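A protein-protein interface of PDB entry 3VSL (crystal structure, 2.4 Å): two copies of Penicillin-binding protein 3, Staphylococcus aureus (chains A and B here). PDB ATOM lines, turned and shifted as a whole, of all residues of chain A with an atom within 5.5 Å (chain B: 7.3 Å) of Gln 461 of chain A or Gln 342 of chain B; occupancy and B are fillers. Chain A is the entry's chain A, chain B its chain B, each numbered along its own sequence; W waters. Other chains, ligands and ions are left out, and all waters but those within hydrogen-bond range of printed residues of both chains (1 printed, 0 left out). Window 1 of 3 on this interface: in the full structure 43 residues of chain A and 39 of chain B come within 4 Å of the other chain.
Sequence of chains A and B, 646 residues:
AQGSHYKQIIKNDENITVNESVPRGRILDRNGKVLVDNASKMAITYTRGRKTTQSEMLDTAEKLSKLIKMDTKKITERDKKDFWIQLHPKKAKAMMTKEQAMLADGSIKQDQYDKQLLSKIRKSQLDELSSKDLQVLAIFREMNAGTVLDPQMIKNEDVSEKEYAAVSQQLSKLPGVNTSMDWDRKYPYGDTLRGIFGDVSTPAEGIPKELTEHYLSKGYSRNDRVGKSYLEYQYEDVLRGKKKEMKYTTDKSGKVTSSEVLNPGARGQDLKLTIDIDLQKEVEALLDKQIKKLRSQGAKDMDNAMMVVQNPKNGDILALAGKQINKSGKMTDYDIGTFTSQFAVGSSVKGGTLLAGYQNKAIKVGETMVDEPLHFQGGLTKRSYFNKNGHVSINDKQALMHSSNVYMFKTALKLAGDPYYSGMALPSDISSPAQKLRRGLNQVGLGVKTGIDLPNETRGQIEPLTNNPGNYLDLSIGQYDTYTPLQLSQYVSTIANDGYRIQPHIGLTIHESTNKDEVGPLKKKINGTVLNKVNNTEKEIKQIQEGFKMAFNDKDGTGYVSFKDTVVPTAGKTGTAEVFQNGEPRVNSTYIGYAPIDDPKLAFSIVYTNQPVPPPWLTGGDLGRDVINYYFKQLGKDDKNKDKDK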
ATOM      1  N   GLN A 342      -3.664 -19.709 -11.148  1.00  0.00           N
ATOM      2  CA  GLN A 342      -4.444 -20.313 -10.073  1.00  0.00           C
ATOM      3  C   GLN A 342      -4.953 -19.234  -9.116  1.00  0.00           C
ATOM      4  O   GLN A 342      -4.169 -18.443  -8.584  1.00  0.00           O
ATOM      5  CB  GLN A 342      -3.569 -21.320  -9.319  1.00  0.00           C
ATOM      6  CG  GLN A 342      -2.686 -22.190 -10.240  1.00  0.00           C
ATOM      7  CD  GLN A 342      -2.015 -23.353  -9.503  1.00  0.00           C
ATOM      8  OE1 GLN A 342      -1.986 -23.376  -8.274  1.00  0.00           O
ATOM      9  NE2 GLN A 342      -1.488 -24.326 -10.253  1.00  0.00           N
ATOM     10  N   ARG A 459      -3.654 -27.596 -12.609  1.00  0.00           N
ATOM     11  CA  ARG A 459      -4.860 -28.077 -11.948  1.00  0.00           C
ATOM     12  C   ARG A 459      -5.123 -27.280 -10.682  1.00  0.00           C
ATOM     13  O   ARG A 459      -6.153 -27.458 -10.037  1.00  0.00           O
ATOM     14  CB  ARG A 459      -4.728 -29.560 -11.601  1.00  0.00           C
ATOM     15  CG  ARG A 459      -3.884 -29.765 -10.372  1.00  0.00           C
ATOM     16  CD  ARG A 459      -3.161 -31.080 -10.355  1.00  0.00           C
ATOM     17  NE  ARG A 459      -2.285 -31.116  -9.187  1.00  0.00           N
ATOM     18  CZ  ARG A 459      -2.265 -32.107  -8.310  1.00  0.00           C
ATOM     19  NH1 ARG A 459      -3.069 -33.147  -8.483  1.00  0.00           N
ATOM     20  NH2 ARG A 459      -1.448 -32.044  -7.266  1.00  0.00           N
ATOM     21  N   GLY A 460      -4.192 -26.417 -10.302  1.00  0.00           N
ATOM     22  CA  GLY A 460      -4.365 -25.633  -9.093  1.00  0.00           C
ATOM     23  C   GLY A 460      -3.487 -26.051  -7.927  1.00  0.00           C
ATOM     24  O   GLY A 460      -2.881 -27.125  -7.928  1.00  0.00           O
ATOM     25  N   GLN A 461      -3.400 -25.191  -6.918  1.00  0.00           N
ATOM     26  CA  GLN A 461      -2.587 -25.477  -5.743  1.00  0.00           C
ATOM     27  C   GLN A 461      -3.348 -26.450  -4.828  1.00  0.00           C
ATOM     28  O   GLN A 461      -4.482 -26.171  -4.433  1.00  0.00           O
ATOM     29  CB  GLN A 461      -2.284 -24.190  -5.009  1.00  0.00           C
ATOM     30  CG  GLN A 461      -1.844 -24.417  -3.587  1.00  0.00           C
ATOM     31  CD  GLN A 461      -1.593 -23.128  -2.849  1.00  0.00           C
ATOM     32  OE1 GLN A 461      -2.508 -22.547  -2.259  1.00  0.00           O
ATOM     33  NE2 GLN A 461      -0.346 -22.666  -2.884  1.00  0.00           N
ATOM     34  N   ILE A 462      -2.746 -27.597  -4.514  1.00  0.00           N
ATOM     35  CA  ILE A 462      -3.417 -28.599  -3.695  1.00  0.00           C
ATOM     36  C   ILE A 462      -2.587 -29.040  -2.477  1.00  0.00           C
ATOM     37  O   ILE A 462      -1.816 -30.006  -2.554  1.00  0.00           O
ATOM     38  CB  ILE A 462      -3.780 -29.857  -4.508  1.00  0.00           C
ATOM     39  CG1 ILE A 462      -4.432 -29.497  -5.847  1.00  0.00           C
ATOM     40  CG2 ILE A 462      -4.698 -30.738  -3.695  1.00  0.00           C
ATOM     41  CD1 ILE A 462      -5.096 -30.705  -6.499  1.00  0.00           C
ATOM     42  N   GLU A 463      -2.771 -28.352  -1.351  1.00  0.00           N
ATOM     43  CA  GLU A 463      -1.956 -28.589  -0.161  1.00  0.00           C
ATOM     44  C   GLU A 463      -2.521 -29.708   0.726  1.00  0.00           C
ATOM     45  O   GLU A 463      -3.730 -29.974   0.709  1.00  0.00           O
ATOM     46  CB  GLU A 463      -1.829 -27.288   0.635  1.00  0.00           C
ATOM     47  CG  GLU A 463      -1.088 -26.165  -0.077  1.00  0.00           C
ATOM     48  CD  GLU A 463      -1.555 -24.784   0.373  1.00  0.00           C
ATOM     49  OE1 GLU A 463      -0.726 -24.025   0.913  1.00  0.00           O
ATOM     50  OE2 GLU A 463      -2.748 -24.450   0.190  1.00  0.00           O
ATOM     51  N   TYR A 480      -9.564 -22.516   0.161  1.00  0.00           N
ATOM     52  CA  TYR A 480      -8.289 -23.204   0.367  1.00  0.00           C
ATOM     53  C   TYR A 480      -7.571 -23.496  -0.954  1.00  0.00           C
ATOM     54  O   TYR A 480      -6.470 -23.000  -1.195  1.00  0.00           O
ATOM     55  CB  TYR A 480      -8.468 -24.487   1.173  1.00  0.00           C
ATOM     56  CG  TYR A 480      -7.164 -25.073   1.664  1.00  0.00           C
ATOM     57  CD1 TYR A 480      -6.229 -24.294   2.320  1.00  0.00           C
ATOM     58  CD2 TYR A 480      -6.876 -26.411   1.486  1.00  0.00           C
ATOM     59  CE1 TYR A 480      -5.043 -24.828   2.775  1.00  0.00           C
ATOM     60  CE2 TYR A 480      -5.685 -26.959   1.940  1.00  0.00           C
ATOM     61  CZ  TYR A 480      -4.775 -26.160   2.588  1.00  0.00           C
ATOM     62  OH  TYR A 480      -3.594 -26.697   3.048  1.00  0.00           O
ATOM     63  N   ASP A 481      -8.190 -24.314  -1.796  1.00  0.00           N
ATOM     64  CA  ASP A 481      -7.527 -24.764  -2.992  1.00  0.00           C
ATOM     65  C   ASP A 481      -7.756 -23.755  -4.100  1.00  0.00           C
ATOM     66  O   ASP A 481      -8.879 -23.292  -4.292  1.00  0.00           O
ATOM     67  CB  ASP A 481      -8.056 -26.149  -3.381  1.00  0.00           C
ATOM     68  CG  ASP A 481      -7.447 -27.260  -2.544  1.00  0.00           C
ATOM     69  OD1 ASP A 481      -6.722 -26.951  -1.559  1.00  0.00           O
ATOM     70  OD2 ASP A 481      -7.673 -28.441  -2.880  1.00  0.00           O
ATOM     71  N   THR A 482      -6.692 -23.372  -4.800  1.00  0.00           N
ATOM     72  CA  THR A 482      -6.838 -22.437  -5.924  1.00  0.00           C
ATOM     73  C   THR A 482      -7.237 -23.174  -7.216  1.00  0.00           C
ATOM     74  O   THR A 482      -6.713 -24.255  -7.516  1.00  0.00           O
ATOM     75  CB  THR A 482      -5.562 -21.577  -6.162  1.00  0.00           C
ATOM     76  OG1 THR A 482      -4.455 -22.428  -6.465  1.00  0.00           O
ATOM     77  CG2 THR A 482      -5.216 -20.743  -4.934  1.00  0.00           C
ATOM     78  N   ASN B 304       6.158 -25.047   5.491  1.00  0.00           N
ATOM     79  CA  ASN B 304       6.705 -25.959   4.504  1.00  0.00           C
ATOM     80  C   ASN B 304       8.219 -26.085   4.654  1.00  0.00           C
ATOM     81  O   ASN B 304       8.909 -25.116   4.983  1.00  0.00           O
ATOM     82  CB  ASN B 304       6.349 -25.500   3.080  1.00  0.00           C
ATOM     83  CG  ASN B 304       4.865 -25.677   2.749  1.00  0.00           C
ATOM     84  OD1 ASN B 304       4.272 -26.721   3.037  1.00  0.00           O
ATOM     85  ND2 ASN B 304       4.265 -24.658   2.124  1.00  0.00           N
ATOM     86  N   TYR B 334       4.551 -34.439   2.763  1.00  0.00           N
ATOM     87  CA  TYR B 334       4.361 -33.560   1.617  1.00  0.00           C
ATOM     88  C   TYR B 334       5.472 -33.733   0.614  1.00  0.00           C
ATOM     89  O   TYR B 334       5.962 -32.756   0.051  1.00  0.00           O
ATOM     90  CB  TYR B 334       4.304 -32.097   2.055  1.00  0.00           C
ATOM     91  CG  TYR B 334       3.623 -31.200   1.050  1.00  0.00           C
ATOM     92  CD1 TYR B 334       2.998 -31.731  -0.078  1.00  0.00           C
ATOM     93  CD2 TYR B 334       3.598 -29.826   1.225  1.00  0.00           C
ATOM     94  CE1 TYR B 334       2.361 -30.913  -1.012  1.00  0.00           C
ATOM     95  CE2 TYR B 334       2.976 -28.990   0.293  1.00  0.00           C
ATOM     96  CZ  TYR B 334       2.354 -29.541  -0.823  1.00  0.00           C
ATOM     97  OH  TYR B 334       1.731 -28.718  -1.738  1.00  0.00           O
ATOM     98  N   GLY B 337       5.100 -32.252  -2.776  1.00  0.00           N
ATOM     99  CA  GLY B 337       5.377 -30.825  -2.820  1.00  0.00           C
ATOM    100  C   GLY B 337       6.615 -30.415  -3.602  1.00  0.00           C
ATOM    101  O   GLY B 337       6.634 -29.351  -4.216  1.00  0.00           O
ATOM    102  N   PHE B 339       7.674 -31.256  -6.472  1.00  0.00           N
ATOM    103  CA  PHE B 339       7.495 -31.010  -7.913  1.00  0.00           C
ATOM    104  C   PHE B 339       6.115 -30.480  -8.284  1.00  0.00           C
ATOM    105  O   PHE B 339       5.878 -30.111  -9.434  1.00  0.00           O
ATOM    106  CB  PHE B 339       7.791 -32.268  -8.732  1.00  0.00           C
ATOM    107  CG  PHE B 339       6.919 -33.448  -8.375  1.00  0.00           C
ATOM    108  CD1 PHE B 339       7.276 -34.299  -7.352  1.00  0.00           C
ATOM    109  CD2 PHE B 339       5.755 -33.711  -9.075  1.00  0.00           C
ATOM    110  CE1 PHE B 339       6.489 -35.387  -7.006  1.00  0.00           C
ATOM    111  CE2 PHE B 339       4.955 -34.807  -8.734  1.00  0.00           C
ATOM    112  CZ  PHE B 339       5.331 -35.635  -7.688  1.00  0.00           C
ATOM    113  N   THR B 340       5.204 -30.457  -7.311  1.00  0.00           N
ATOM    114  CA  THR B 340       3.836 -30.036  -7.570  1.00  0.00           C
ATOM    115  C   THR B 340       3.593 -28.626  -7.059  1.00  0.00           C
ATOM    116  O   THR B 340       2.617 -27.969  -7.444  1.00  0.00           O
ATOM    117  CB  THR B 340       2.809 -30.995  -6.956  1.00  0.00           C
ATOM    118  OG1 THR B 340       2.886 -30.932  -5.529  1.00  0.00           O
ATOM    119  CG2 THR B 340       3.076 -32.399  -7.402  1.00  0.00           C
ATOM    120  N   SER B 341       4.476 -28.146  -6.190  1.00  0.00           N
ATOM    121  CA  SER B 341       4.215 -26.850  -5.573  1.00  0.00           C
ATOM    122  C   SER B 341       5.176 -25.691  -5.911  1.00  0.00           C
ATOM    123  O   SER B 341       6.357 -25.879  -6.235  1.00  0.00           O
ATOM    124  CB  SER B 341       3.986 -27.015  -4.065  1.00  0.00           C
ATOM    125  OG  SER B 341       2.801 -27.770  -3.843  1.00  0.00           O
ATOM    126  N   GLN B 342       4.632 -24.485  -5.796  1.00  0.00           N
ATOM    127  CA  GLN B 342       5.166 -23.282  -6.427  1.00  0.00           C
ATOM    128  C   GLN B 342       5.673 -22.292  -5.373  1.00  0.00           C
ATOM    129  O   GLN B 342       4.872 -21.669  -4.677  1.00  0.00           O
ATOM    130  CB  GLN B 342       4.035 -22.639  -7.251  1.00  0.00           C
ATOM    131  CG  GLN B 342       2.805 -23.585  -7.540  1.00  0.00           C
ATOM    132  CD  GLN B 342       1.839 -23.786  -6.343  1.00  0.00           C
ATOM    133  OE1 GLN B 342       1.178 -24.832  -6.216  1.00  0.00           O
ATOM    134  NE2 GLN B 342       1.754 -22.779  -5.479  1.00  0.00           N
ATOM    135  N   PHE B 343       6.987 -22.125  -5.251  1.00  0.00           N
ATOM    136  CA  PHE B 343       7.510 -21.316  -4.145  1.00  0.00           C
ATOM    137  C   PHE B 343       8.458 -20.187  -4.561  1.00  0.00           C
ATOM    138  O   PHE B 343       9.444 -20.413  -5.290  1.00  0.00           O
ATOM    139  CB  PHE B 343       8.184 -22.224  -3.116  1.00  0.00           C
ATOM    140  CG  PHE B 343       7.261 -23.271  -2.546  1.00  0.00           C
ATOM    141  CD1 PHE B 343       5.971 -22.932  -2.165  1.00  0.00           C
ATOM    142  CD2 PHE B 343       7.669 -24.592  -2.398  1.00  0.00           C
ATOM    143  CE1 PHE B 343       5.101 -23.886  -1.640  1.00  0.00           C
ATOM    144  CE2 PHE B 343       6.801 -25.560  -1.869  1.00  0.00           C
ATOM    145  CZ  PHE B 343       5.512 -25.199  -1.487  1.00  0.00           C
ATOM    146  N   ALA B 344       8.163 -18.971  -4.094  1.00  0.00           N
ATOM    147  CA  ALA B 344       9.064 -17.840  -4.310  1.00  0.00           C
ATOM    148  C   ALA B 344      10.384 -18.146  -3.605  1.00  0.00           C
ATOM    149  O   ALA B 344      10.406 -18.576  -2.430  1.00  0.00           O
ATOM    150  CB  ALA B 344       8.446 -16.540  -3.795  1.00  0.00           C
ATOM    151  N   THR B 458       4.369 -28.972 -11.872  1.00  0.00           N
ATOM    152  CA  THR B 458       3.990 -27.612 -12.229  1.00  0.00           C
ATOM    153  C   THR B 458       5.224 -26.826 -12.626  1.00  0.00           C
ATOM    154  O   THR B 458       6.325 -27.081 -12.134  1.00  0.00           O
ATOM    155  CB  THR B 458       3.322 -26.900 -11.043  1.00  0.00           C
ATOM    156  OG1 THR B 458       4.263 -26.808  -9.966  1.00  0.00           O
ATOM    157  CG2 THR B 458       2.110 -27.687 -10.578  1.00  0.00           C
ATOM    158  N   ARG B 459       5.061 -25.866 -13.516  1.00  0.00           N
ATOM    159  CA  ARG B 459       6.250 -25.182 -13.999  1.00  0.00           C
ATOM    160  C   ARG B 459       6.446 -23.871 -13.292  1.00  0.00           C
ATOM    161  O   ARG B 459       7.370 -23.139 -13.620  1.00  0.00           O
ATOM    162  CB  ARG B 459       6.162 -24.901 -15.494  1.00  0.00           C
ATOM    163  CG  ARG B 459       5.127 -23.869 -15.809  1.00  0.00           C
ATOM    164  CD  ARG B 459       4.863 -23.758 -17.252  1.00  0.00           C
ATOM    165  NE  ARG B 459       4.154 -22.513 -17.480  1.00  0.00           N
ATOM    166  CZ  ARG B 459       4.320 -21.763 -18.554  1.00  0.00           C
ATOM    167  NH1 ARG B 459       5.148 -22.181 -19.493  1.00  0.00           N
ATOM    168  NH2 ARG B 459       3.664 -20.607 -18.677  1.00  0.00           N
ATOM    169  N   GLY B 460       5.546 -23.555 -12.364  1.00  0.00           N
ATOM    170  CA  GLY B 460       5.614 -22.305 -11.617  1.00  0.00           C
ATOM    171  C   GLY B 460       4.711 -21.204 -12.151  1.00  0.00           C
ATOM    172  O   GLY B 460       4.402 -21.179 -13.347  1.00  0.00           O
ATOM    173  N   GLN B 461       4.287 -20.293 -11.276  1.00  0.00           N
ATOM    174  CA  GLN B 461       3.387 -19.218 -11.680  1.00  0.00           C
ATOM    175  C   GLN B 461       4.178 -18.160 -12.444  1.00  0.00           C
ATOM    176  O   GLN B 461       5.181 -17.632 -11.940  1.00  0.00           O
ATOM    177  CB  GLN B 461       2.668 -18.620 -10.471  1.00  0.00           C
ATOM    178  CG  GLN B 461       1.423 -17.781 -10.834  1.00  0.00           C
ATOM    179  CD  GLN B 461       0.135 -18.597 -11.071  1.00  0.00           C
ATOM    180  OE1 GLN B 461       0.113 -19.553 -11.854  1.00  0.00           O
ATOM    181  NE2 GLN B 461      -0.951 -18.195 -10.398  1.00  0.00           N
ATOM    182  N   THR B 482       7.835 -17.945  -9.374  1.00  0.00           N
ATOM    183  CA  THR B 482       7.949 -19.115  -8.523  1.00  0.00           C
ATOM    184  C   THR B 482       8.399 -20.384  -9.260  1.00  0.00           C
ATOM    185  O   THR B 482       7.940 -20.691 -10.373  1.00  0.00           O
ATOM    186  CB  THR B 482       6.624 -19.374  -7.835  1.00  0.00           C
ATOM    187  OG1 THR B 482       5.582 -19.357  -8.823  1.00  0.00           O
ATOM    188  CG2 THR B 482       6.365 -18.291  -6.795  1.00  0.00           C
ATOM    189  N   TYR B 483       9.316 -21.111  -8.632  1.00  0.00           N
ATOM    190  CA  TYR B 483       9.740 -22.398  -9.146  1.00  0.00           C
ATOM    191  C   TYR B 483       9.361 -23.502  -8.163  1.00  0.00           C
ATOM    192  O   TYR B 483       8.718 -23.253  -7.138  1.00  0.00           O
ATOM    193  CB  TYR B 483      11.246 -22.382  -9.401  1.00  0.00           C
ATOM    194  CG  TYR B 483      11.667 -21.236 -10.279  1.00  0.00           C
ATOM    195  CD1 TYR B 483      11.324 -21.217 -11.621  1.00  0.00           C
ATOM    196  CD2 TYR B 483      12.391 -20.163  -9.769  1.00  0.00           C
ATOM    197  CE1 TYR B 483      11.696 -20.167 -12.439  1.00  0.00           C
ATOM    198  CE2 TYR B 483      12.768 -19.106 -10.581  1.00  0.00           C
ATOM    199  CZ  TYR B 483      12.413 -19.115 -11.918  1.00  0.00           C
ATOM    200  OH  TYR B 483      12.777 -18.073 -12.741  1.00  0.00           O
ATOM    201  N   THR B 484       9.759 -24.724  -8.490  1.00  0.00           N
ATOM    202  CA  THR B 484       9.595 -25.854  -7.580  1.00  0.00           C
ATOM    203  C   THR B 484      10.977 -26.218  -7.019  1.00  0.00           C
ATOM    204  O   THR B 484      11.999 -25.835  -7.606  1.00  0.00           O
ATOM    205  CB  THR B 484       9.003 -27.074  -8.318  1.00  0.00           C
ATOM    206  OG1 THR B 484      10.058 -27.765  -8.994  1.00  0.00           O
ATOM    207  CG2 THR B 484       7.938 -26.648  -9.332  1.00  0.00           C
ATOM    208  N   PRO B 485      11.017 -26.941  -5.883  1.00  0.00           N
ATOM    209  CA  PRO B 485      12.291 -27.518  -5.437  1.00  0.00           C
ATOM    210  C   PRO B 485      12.954 -28.354  -6.534  1.00  0.00           C
ATOM    211  O   PRO B 485      14.150 -28.177  -6.785  1.00  0.00           O
ATOM    212  CB  PRO B 485      11.864 -28.414  -4.272  1.00  0.00           C
ATOM    213  CG  PRO B 485      10.706 -27.684  -3.673  1.00  0.00           C
ATOM    214  CD  PRO B 485       9.966 -27.067  -4.848  1.00  0.00           C
ATOM    215  N   GLN B 487      12.654 -28.086  -9.817  1.00  0.00           N
ATOM    216  CA  GLN B 487      13.232 -27.090 -10.736  1.00  0.00           C
ATOM    217  C   GLN B 487      14.607 -26.536 -10.258  1.00  0.00           C
ATOM    218  O   GLN B 487      15.518 -26.348 -11.072  1.00  0.00           O
ATOM    219  CB  GLN B 487      12.236 -25.944 -11.040  1.00  0.00           C
ATOM    220  CG  GLN B 487      11.185 -26.232 -12.122  1.00  0.00           C
ATOM    221  CD  GLN B 487      10.231 -25.039 -12.402  1.00  0.00           C
ATOM    222  OE1 GLN B 487       9.546 -24.551 -11.497  1.00  0.00           O
ATOM    223  NE2 GLN B 487      10.185 -24.583 -13.663  1.00  0.00           N
ATOM    224  N   ASN B 588      10.963 -16.521   2.800  1.00  0.00           N
ATOM    225  CA  ASN B 588      11.402 -17.814   2.318  1.00  0.00           C
ATOM    226  C   ASN B 588      12.930 -17.969   2.250  1.00  0.00           C
ATOM    227  O   ASN B 588      13.662 -17.057   1.838  1.00  0.00           O
ATOM    228  CB  ASN B 588      10.733 -18.117   0.986  1.00  0.00           C
ATOM    229  CG  ASN B 588       9.468 -18.916   1.150  1.00  0.00           C
ATOM    230  OD1 ASN B 588       9.395 -20.037   0.675  1.00  0.00           O
ATOM    231  ND2 ASN B 588       8.475 -18.361   1.840  1.00  0.00           N
ATOM    232  N   THR B 609       9.689 -22.440   3.814  1.00  0.00           N
ATOM    233  CA  THR B 609       8.738 -21.380   3.517  1.00  0.00           C
ATOM    234  C   THR B 609       8.142 -20.720   4.756  1.00  0.00           C
ATOM    235  O   THR B 609       7.837 -21.384   5.762  1.00  0.00           O
ATOM    236  CB  THR B 609       7.656 -21.820   2.512  1.00  0.00           C
ATOM    237  OG1 THR B 609       6.517 -22.336   3.195  1.00  0.00           O
ATOM    238  CG2 THR B 609       8.205 -22.883   1.574  1.00  0.00           C
HETATM  239  O   HOH W   1       0.191 -27.776  -5.173  1.00  0.00           O
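The side-chain amide nitrogen of Gln 342 of chain A lies close to the backbone NH of Gly 460 of chain A, 3.4 Å away.
OE1 of Gln 342 of chain A sits at hydrogen-bond distance from N of Gln 461 of chain A (2.7 Å).
The side-chain amide oxygen (OE1) of Gln 342 of chain A sits close to the side-chain hydroxyl (OG1) of Thr 482 of chain A, 3.2 Å away.
OE2 of Glu 463 of chain A sits close to OE1 of Gln 461 of chain A.
OH of Tyr 334 of chain B sits at hydrogen-bond distance from OG of Ser 341 of chain B (2.5 Å).
N of Gln 461 of chain B sits at hydrogen-bond distance from OG1 of Thr 482 of chain B.
Water W1 lies within hydrogen-bond range of the side-chain hydroxyl (OG) of Ser 341 of chain B, the backbone NH (N) of Ile 462 of chain A, the side-chain amide oxygen (OE1) of Gln 342 of chain B and the backbone carbonyl oxygen (O) of Thr 340 of chain B.
The backbone NH (N) of Gln 342 of chain A lies close to the side-chain amide nitrogen (NE2) of Gln 461 of chain B (3.2 Å).
The side-chain amide nitrogen (NE2) of Gln 461 of chain A lies close to the side-chain amide nitrogen (NE2) of Gln 342 of chain B (3.3 Å).
Of the 9 printed residues of chain A, 3 touch a printed residue of chain B.
Of the 20 printed residues of chain B, 3 touch a printed residue of chain A.
Hydrophobic or aromatic side chains of chain B within 4 Å of the printed part of chain A: Tyr 334.
Among the printed residues, no Asp or Glu carboxylate lies within 4 Å of a Lys or Arg side-chain nitrogen of the other chain.
Gln 461 of chain A touches just one residue of chain B: Gln 342 (3.3 Å).
Printed residues of chain A within 4 Å of Tyr 334 of chain B: Ile 462 (3.9 Å).
Of the printed residues of chain A, Gln 461 of chain B touches Gln 342.
Thr 458 of chain B touches none of the printed residues of chain A.
Asn 588 of chain B touches none of the printed residues of chain A.
The nearest printed residue of chain B that does not touch Gln 461 of chain A is Phe 343 of chain B (5.7 Å).
The nearest residue of chain A that does not touch Gln 342 of chain B is Gln 342 of chain A (4.05 Å).
Gln 342 of chain A touches Gln 461 of chain B, and with the chains exchanged Gln 461 of chain A touches Gln 342 of chain B.
Of the 3 pairs that touch across the chains among the printed residues, 2 have their exchanged pair printed and touching as well.
Among the printed residues, pairs that only touch across the chains: Ile 462 of chain A with Tyr 334 of chain B (3.9 Å).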
